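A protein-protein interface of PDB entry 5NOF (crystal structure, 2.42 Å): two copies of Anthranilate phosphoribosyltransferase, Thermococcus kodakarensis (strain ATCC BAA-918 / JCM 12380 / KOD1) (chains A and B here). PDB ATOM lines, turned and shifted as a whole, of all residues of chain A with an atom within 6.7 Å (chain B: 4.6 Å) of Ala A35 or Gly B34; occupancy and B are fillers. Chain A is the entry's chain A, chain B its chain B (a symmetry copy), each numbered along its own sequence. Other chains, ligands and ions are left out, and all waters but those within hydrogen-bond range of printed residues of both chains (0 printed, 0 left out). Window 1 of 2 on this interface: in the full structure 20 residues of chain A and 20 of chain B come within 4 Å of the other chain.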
ATOM      1  N   LEU A   4     -18.027  12.202 -10.950  1.00  0.00           N
ATOM      2  CA  LEU A   4     -18.549  12.324  -9.590  1.00  0.00           C
ATOM      3  C   LEU A   4     -17.554  13.043  -8.692  1.00  0.00           C
ATOM      4  O   LEU A   4     -17.925  13.974  -7.960  1.00  0.00           O
ATOM      5  CB  LEU A   4     -18.892  10.956  -8.997  1.00  0.00           C
ATOM      6  CG  LEU A   4     -19.584  10.931  -7.642  1.00  0.00           C
ATOM      7  CD1 LEU A   4     -20.880  11.712  -7.716  1.00  0.00           C
ATOM      8  CD2 LEU A   4     -19.808   9.480  -7.201  1.00  0.00           C
ATOM      9  N   ILE A   7     -17.580  16.755  -9.472  1.00  0.00           N
ATOM     10  CA  ILE A   7     -18.788  17.392  -8.879  1.00  0.00           C
ATOM     11  C   ILE A   7     -18.689  17.597  -7.353  1.00  0.00           C
ATOM     12  O   ILE A   7     -19.014  18.657  -6.833  1.00  0.00           O
ATOM     13  CB  ILE A   7     -20.065  16.563  -9.193  1.00  0.00           C
ATOM     14  CG1 ILE A   7     -20.388  16.583 -10.680  1.00  0.00           C
ATOM     15  CG2 ILE A   7     -21.276  17.044  -8.389  1.00  0.00           C
ATOM     16  CD1 ILE A   7     -21.217  15.388 -11.113  1.00  0.00           C
ATOM     17  N   VAL A   8     -18.272  16.553  -6.647  1.00  0.00           N
ATOM     18  CA  VAL A   8     -18.139  16.585  -5.181  1.00  0.00           C
ATOM     19  C   VAL A   8     -17.073  17.594  -4.711  1.00  0.00           C
ATOM     20  O   VAL A   8     -17.201  18.177  -3.643  1.00  0.00           O
ATOM     21  CB  VAL A   8     -17.830  15.164  -4.650  1.00  0.00           C
ATOM     22  CG1 VAL A   8     -17.265  15.179  -3.260  1.00  0.00           C
ATOM     23  CG2 VAL A   8     -19.077  14.276  -4.748  1.00  0.00           C
ATOM     24  N   GLY A  30     -28.345   2.005 -10.021  1.00  0.00           N
ATOM     25  CA  GLY A  30     -29.092   3.003  -9.247  1.00  0.00           C
ATOM     26  C   GLY A  30     -28.280   3.722  -8.185  1.00  0.00           C
ATOM     27  O   GLY A  30     -28.499   4.911  -7.934  1.00  0.00           O
ATOM     28  N   VAL A  31     -27.338   3.000  -7.573  1.00  0.00           N
ATOM     29  CA  VAL A  31     -26.450   3.548  -6.542  1.00  0.00           C
ATOM     30  C   VAL A  31     -25.666   4.754  -7.074  1.00  0.00           C
ATOM     31  O   VAL A  31     -25.576   5.775  -6.409  1.00  0.00           O
ATOM     32  CB  VAL A  31     -25.485   2.454  -5.976  1.00  0.00           C
ATOM     33  CG1 VAL A  31     -24.521   2.995  -4.906  1.00  0.00           C
ATOM     34  CG2 VAL A  31     -26.294   1.279  -5.429  1.00  0.00           C
ATOM     35  N   LEU A  32     -25.119   4.628  -8.270  1.00  0.00           N
ATOM     36  CA  LEU A  32     -24.298   5.681  -8.852  1.00  0.00           C
ATOM     37  C   LEU A  32     -25.164   6.834  -9.369  1.00  0.00           C
ATOM     38  O   LEU A  32     -24.780   8.014  -9.273  1.00  0.00           O
ATOM     39  CB  LEU A  32     -23.451   5.112  -9.982  1.00  0.00           C
ATOM     40  CG  LEU A  32     -22.172   5.854 -10.307  1.00  0.00           C
ATOM     41  CD1 LEU A  32     -21.141   5.663  -9.203  1.00  0.00           C
ATOM     42  CD2 LEU A  32     -21.645   5.373 -11.654  1.00  0.00           C
ATOM     43  N   ILE A  33     -26.327   6.497  -9.917  1.00  0.00           N
ATOM     44  CA  ILE A  33     -27.287   7.508 -10.366  1.00  0.00           C
ATOM     45  C   ILE A  33     -27.707   8.362  -9.175  1.00  0.00           C
ATOM     46  O   ILE A  33     -27.740   9.579  -9.283  1.00  0.00           O
ATOM     47  CB  ILE A  33     -28.537   6.890 -11.044  1.00  0.00           C
ATOM     48  CG1 ILE A  33     -28.141   6.173 -12.349  1.00  0.00           C
ATOM     49  CG2 ILE A  33     -29.599   7.963 -11.326  1.00  0.00           C
ATOM     50  CD1 ILE A  33     -29.118   5.111 -12.776  1.00  0.00           C
ATOM     51  N   GLY A  34     -28.019   7.722  -8.051  1.00  0.00           N
ATOM     52  CA  GLY A  34     -28.419   8.433  -6.840  1.00  0.00           C
ATOM     53  C   GLY A  34     -27.336   9.396  -6.386  1.00  0.00           C
ATOM     54  O   GLY A  34     -27.605  10.570  -6.090  1.00  0.00           O
ATOM     55  N   ALA A  35     -26.103   8.893  -6.346  1.00  0.00           N
ATOM     56  CA  ALA A  35     -24.944   9.702  -5.982  1.00  0.00           C
ATOM     57  C   ALA A  35     -24.800  10.904  -6.889  1.00  0.00           C
ATOM     58  O   ALA A  35     -24.553  12.014  -6.404  1.00  0.00           O
ATOM     59  CB  ALA A  35     -23.683   8.873  -6.024  1.00  0.00           C
ATOM     60  N   TYR A  36     -24.963  10.695  -8.195  1.00  0.00           N
ATOM     61  CA  TYR A  36     -24.840  11.788  -9.161  1.00  0.00           C
ATOM     62  C   TYR A  36     -25.924  12.838  -8.973  1.00  0.00           C
ATOM     63  O   TYR A  36     -25.631  14.032  -8.937  1.00  0.00           O
ATOM     64  CB  TYR A  36     -24.817  11.277 -10.619  1.00  0.00           C
ATOM     65  CG  TYR A  36     -23.427  10.908 -11.125  1.00  0.00           C
ATOM     66  CD1 TYR A  36     -22.443  11.879 -11.265  1.00  0.00           C
ATOM     67  CD2 TYR A  36     -23.102   9.587 -11.474  1.00  0.00           C
ATOM     68  CE1 TYR A  36     -21.177  11.561 -11.734  1.00  0.00           C
ATOM     69  CE2 TYR A  36     -21.838   9.255 -11.944  1.00  0.00           C
ATOM     70  CZ  TYR A  36     -20.880  10.242 -12.073  1.00  0.00           C
ATOM     71  OH  TYR A  36     -19.620   9.921 -12.525  1.00  0.00           O
ATOM     72  N   LEU A  37     -27.169  12.396  -8.839  1.00  0.00           N
ATOM     73  CA  LEU A  37     -28.300  13.314  -8.750  1.00  0.00           C
ATOM     74  C   LEU A  37     -28.239  14.145  -7.482  1.00  0.00           C
ATOM     75  O   LEU A  37     -28.402  15.364  -7.542  1.00  0.00           O
ATOM     76  CB  LEU A  37     -29.630  12.567  -8.868  1.00  0.00           C
ATOM     77  CG  LEU A  37     -29.891  11.867 -10.205  1.00  0.00           C
ATOM     78  CD1 LEU A  37     -31.346  11.414 -10.318  1.00  0.00           C
ATOM     79  CD2 LEU A  37     -29.503  12.728 -11.396  1.00  0.00           C
ATOM     80  N   ALA A  38     -27.950  13.489  -6.359  1.00  0.00           N
ATOM     81  CA  ALA A  38     -27.833  14.175  -5.080  1.00  0.00           C
ATOM     82  C   ALA A  38     -26.654  15.145  -5.055  1.00  0.00           C
ATOM     83  O   ALA A  38     -26.800  16.268  -4.594  1.00  0.00           O
ATOM     84  CB  ALA A  38     -27.716  13.171  -3.939  1.00  0.00           C
ATOM     85  N   ALA A  39     -25.503  14.730  -5.580  1.00  0.00           N
ATOM     86  CA  ALA A  39     -24.286  15.560  -5.563  1.00  0.00           C
ATOM     87  C   ALA A  39     -24.403  16.808  -6.427  1.00  0.00           C
ATOM     88  O   ALA A  39     -23.972  17.905  -6.055  1.00  0.00           O
ATOM     89  CB  ALA A  39     -23.088  14.737  -6.010  1.00  0.00           C
ATOM     90  N   LEU A  40     -24.979  16.624  -7.599  1.00  0.00           N
ATOM     91  CA  LEU A  40     -25.201  17.706  -8.547  1.00  0.00           C
ATOM     92  C   LEU A  40     -26.230  18.702  -7.982  1.00  0.00           C
ATOM     93  O   LEU A  40     -26.095  19.915  -8.162  1.00  0.00           O
ATOM     94  CB  LEU A  40     -25.664  17.091  -9.874  1.00  0.00           C
ATOM     95  CG  LEU A  40     -25.685  17.916 -11.146  1.00  0.00           C
ATOM     96  CD1 LEU A  40     -24.389  18.678 -11.334  1.00  0.00           C
ATOM     97  CD2 LEU A  40     -25.946  16.986 -12.316  1.00  0.00           C
ATOM     98  N   VAL A 158     -35.030   5.923  -9.332  1.00  0.00           N
ATOM     99  CA  VAL A 158     -34.058   6.594  -8.479  1.00  0.00           C
ATOM    100  C   VAL A 158     -34.581   7.958  -8.055  1.00  0.00           C
ATOM    101  O   VAL A 158     -34.389   8.353  -6.916  1.00  0.00           O
ATOM    102  CB  VAL A 158     -32.683   6.692  -9.154  1.00  0.00           C
ATOM    103  CG1 VAL A 158     -31.697   7.465  -8.282  1.00  0.00           C
ATOM    104  CG2 VAL A 158     -32.152   5.286  -9.440  1.00  0.00           C
ATOM    105  N   LEU A 162     -35.408   8.857  -3.993  1.00  0.00           N
ATOM    106  CA  LEU A 162     -34.688   9.988  -3.384  1.00  0.00           C
ATOM    107  C   LEU A 162     -35.638  11.030  -2.820  1.00  0.00           C
ATOM    108  O   LEU A 162     -35.375  11.595  -1.744  1.00  0.00           O
ATOM    109  CB  LEU A 162     -33.754  10.687  -4.394  1.00  0.00           C
ATOM    110  CG  LEU A 162     -32.478  10.012  -4.905  1.00  0.00           C
ATOM    111  CD1 LEU A 162     -31.535  11.051  -5.508  1.00  0.00           C
ATOM    112  CD2 LEU A 162     -31.785   9.168  -3.850  1.00  0.00           C
ATOM    113  N   GLY B  30     -29.043   0.732  -1.484  1.00  0.00           N
ATOM    114  CA  GLY B  30     -27.804   1.323  -1.983  1.00  0.00           C
ATOM    115  C   GLY B  30     -27.974   2.673  -2.663  1.00  0.00           C
ATOM    116  O   GLY B  30     -27.098   3.550  -2.545  1.00  0.00           O
ATOM    117  N   VAL B  31     -29.101   2.832  -3.362  1.00  0.00           N
ATOM    118  CA  VAL B  31     -29.431   4.083  -4.063  1.00  0.00           C
ATOM    119  C   VAL B  31     -29.455   5.265  -3.108  1.00  0.00           C
ATOM    120  O   VAL B  31     -28.892   6.311  -3.403  1.00  0.00           O
ATOM    121  CB  VAL B  31     -30.763   3.995  -4.872  1.00  0.00           C
ATOM    122  CG1 VAL B  31     -31.961   3.756  -3.977  1.00  0.00           C
ATOM    123  CG2 VAL B  31     -30.999   5.264  -5.690  1.00  0.00           C
ATOM    124  N   LEU B  32     -30.081   5.086  -1.952  1.00  0.00           N
ATOM    125  CA  LEU B  32     -30.229   6.173  -0.990  1.00  0.00           C
ATOM    126  C   LEU B  32     -28.919   6.429  -0.236  1.00  0.00           C
ATOM    127  O   LEU B  32     -28.573   7.590   0.062  1.00  0.00           O
ATOM    128  CB  LEU B  32     -31.344   5.842  -0.012  1.00  0.00           C
ATOM    129  CG  LEU B  32     -32.025   7.035   0.641  1.00  0.00           C
ATOM    130  CD1 LEU B  32     -32.894   7.765  -0.376  1.00  0.00           C
ATOM    131  CD2 LEU B  32     -32.839   6.537   1.833  1.00  0.00           C
ATOM    132  N   ILE B  33     -28.198   5.347   0.061  1.00  0.00           N
ATOM    133  CA  ILE B  33     -26.885   5.462   0.691  1.00  0.00           C
ATOM    134  C   ILE B  33     -25.953   6.264  -0.207  1.00  0.00           C
ATOM    135  O   ILE B  33     -25.270   7.155   0.274  1.00  0.00           O
ATOM    136  CB  ILE B  33     -26.243   4.081   1.008  1.00  0.00           C
ATOM    137  CG1 ILE B  33     -27.060   3.342   2.057  1.00  0.00           C
ATOM    138  CG2 ILE B  33     -24.812   4.235   1.516  1.00  0.00           C
ATOM    139  CD1 ILE B  33     -26.872   1.838   2.002  1.00  0.00           C
ATOM    140  N   GLY B  34     -25.938   5.941  -1.498  1.00  0.00           N
ATOM    141  CA  GLY B  34     -25.092   6.643  -2.459  1.00  0.00           C
ATOM    142  C   GLY B  34     -25.416   8.121  -2.490  1.00  0.00           C
ATOM    143  O   GLY B  34     -24.509   8.967  -2.419  1.00  0.00           O
ATOM    144  N   ALA B  35     -26.713   8.428  -2.573  1.00  0.00           N
ATOM    145  CA  ALA B  35     -27.184   9.815  -2.554  1.00  0.00           C
ATOM    146  C   ALA B  35     -26.713  10.551  -1.302  1.00  0.00           C
ATOM    147  O   ALA B  35     -26.244  11.680  -1.393  1.00  0.00           O
ATOM    148  CB  ALA B  35     -28.694   9.868  -2.654  1.00  0.00           C
ATOM    149  N   TYR B  36     -26.830   9.896  -0.148  1.00  0.00           N
ATOM    150  CA  TYR B  36     -26.423  10.514   1.116  1.00  0.00           C
ATOM    151  C   TYR B  36     -24.916  10.764   1.175  1.00  0.00           C
ATOM    152  O   TYR B  36     -24.487  11.851   1.549  1.00  0.00           O
ATOM    153  CB  TYR B  36     -26.882   9.691   2.329  1.00  0.00           C
ATOM    154  CG  TYR B  36     -28.283  10.025   2.825  1.00  0.00           C
ATOM    155  CD1 TYR B  36     -28.579  11.297   3.330  1.00  0.00           C
ATOM    156  CD2 TYR B  36     -29.306   9.070   2.803  1.00  0.00           C
ATOM    157  CE1 TYR B  36     -29.852  11.613   3.783  1.00  0.00           C
ATOM    158  CE2 TYR B  36     -30.582   9.382   3.250  1.00  0.00           C
ATOM    159  CZ  TYR B  36     -30.851  10.658   3.742  1.00  0.00           C
ATOM    160  OH  TYR B  36     -32.109  10.978   4.205  1.00  0.00           O
ATOM    161  N   LEU B  37     -24.123   9.762   0.799  1.00  0.00           N
ATOM    162  CA  LEU B  37     -22.673   9.864   0.893  1.00  0.00           C
ATOM    163  C   LEU B  37     -22.132  10.925  -0.042  1.00  0.00           C
ATOM    164  O   LEU B  37     -21.316  11.767   0.378  1.00  0.00           O
ATOM    165  CB  LEU B  37     -21.995   8.517   0.648  1.00  0.00           C
ATOM    166  CG  LEU B  37     -22.296   7.420   1.688  1.00  0.00           C
ATOM    167  CD1 LEU B  37     -21.379   6.218   1.509  1.00  0.00           C
ATOM    168  CD2 LEU B  37     -22.155   7.954   3.102  1.00  0.00           C
ATOM    169  N   ALA B  38     -22.620  10.923  -1.284  1.00  0.00           N
ATOM    170  CA  ALA B  38     -22.203  11.918  -2.268  1.00  0.00           C
ATOM    171  C   ALA B  38     -22.623  13.333  -1.872  1.00  0.00           C
ATOM    172  O   ALA B  38     -21.820  14.252  -1.959  1.00  0.00           O
ATOM    173  CB  ALA B  38     -22.728  11.565  -3.645  1.00  0.00           C
ATOM    174  N   VAL B 158     -21.352   0.170  -1.655  1.00  0.00           N
ATOM    175  CA  VAL B 158     -21.702   1.506  -2.114  1.00  0.00           C
ATOM    176  C   VAL B 158     -20.460   2.398  -2.143  1.00  0.00           C
ATOM    177  O   VAL B 158     -20.300   3.193  -3.059  1.00  0.00           O
ATOM    178  CB  VAL B 158     -22.819   2.141  -1.250  1.00  0.00           C
ATOM    179  CG1 VAL B 158     -23.116   3.566  -1.714  1.00  0.00           C
ATOM    180  CG2 VAL B 158     -24.062   1.254  -1.262  1.00  0.00           C
ATOM    181  N   LEU B 162     -18.903   3.991  -5.758  1.00  0.00           N
ATOM    182  CA  LEU B 162     -18.773   5.449  -5.862  1.00  0.00           C
ATOM    183  C   LEU B 162     -17.346   5.890  -6.174  1.00  0.00           C
ATOM    184  O   LEU B 162     -17.137   6.816  -6.950  1.00  0.00           O
ATOM    185  CB  LEU B 162     -19.242   6.131  -4.570  1.00  0.00           C
ATOM    186  CG  LEU B 162     -20.746   6.379  -4.365  1.00  0.00           C
ATOM    187  CD1 LEU B 162     -21.660   5.395  -5.075  1.00  0.00           C
ATOM    188  CD2 LEU B 162     -21.066   6.442  -2.882  1.00  0.00           C
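The backbone NH (N) of Leu A4 sits at hydrogen-bond distance from the side-chain hydroxyl (OH) of Tyr A36 (3.2 Å).
Gly A30 touches Val B31.
Val A31 touches Val B158.
Val A31 touches Leu B162 (CG1 to CD1, 3.7 Å).
Gly A34 touches Ala B35 (O to CA, 3.6 Å).
CA of Ala A35 touches O of Gly B34 (3.7 Å).
CB of Ala A38 touches O of Ala B35 (3.3 Å).
CB of Ala B38 touches CB of Ala A39 (3.97 Å).
Val A158 touches Val B31 (CG1 to CG2, 3.5 Å).
CD2 of Leu A162 touches CD1 of Leu B32, 3.9 Å away.
CB of Ala B35 touches CD2 of Leu A162, 3.4 Å away.
Ala A35 touches three residues of chain B.
Gly B34 touches just one residue of chain A: Ala A35.
Of the printed residues of chain A, Gly B30 touches Val A31.
Printed residues of chain B within 4 Å of Gly A34: Ala B35.
Of the printed residues of chain A, Val B158 touches Val A31 (3.5 Å).
Ile A7 touches none of the printed residues of chain B.
The nearest residue of chain B that does not touch Ala A35 is Leu B162 (4.1 Å).
Hydrophobic or aromatic side chains of chain A within 4 Å of the printed part of chain B: Leu A4, Val A8, Val A31, Ala A35, Ala A38, Ala A39, Val A158 and Leu A162.
Of the 11 printed residues of chain B, 8 touch a printed residue of chain A.
Printed residues of chain B that touch a printed residue of chain A: Gly B30, Val B31, Leu B32, Gly B34, Ala B35, Ala B38, Val B158 and Leu B162.
Hydrophobic or aromatic side chains of chain B within 4 Å of the printed part of chain A: Val B31, Leu B32, Ala B35, Ala B38, Val B158 and Leu B162.
Among the printed residues, 16 pairs touch across the chains.
Among the printed residues, no Asp or Glu carboxylate lies within 4 Å of a Lys or Arg side-chain nitrogen of the other chain.
Val A31 touches Val B158, and with the chains exchanged Val A158 touches Val B31.
Val A31 touches Leu B162, but with the chains exchanged Leu A162 does not touch Val B31 (4.1 Å).
Gly A34 touches Ala B35, and with the chains exchanged Ala A35 touches Gly B34.
Leu A162 touches Leu B32, but with the chains exchanged Leu A32 does not touch Leu B162 (4.1 Å).
Positions printed for both chains: 30, 31, 32, 33, 34, 35, 36, 37, 38, 158 and 162.
Of the 16 pairs that touch across the chains among the printed residues, 10 have their exchanged pair printed and touching as well.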
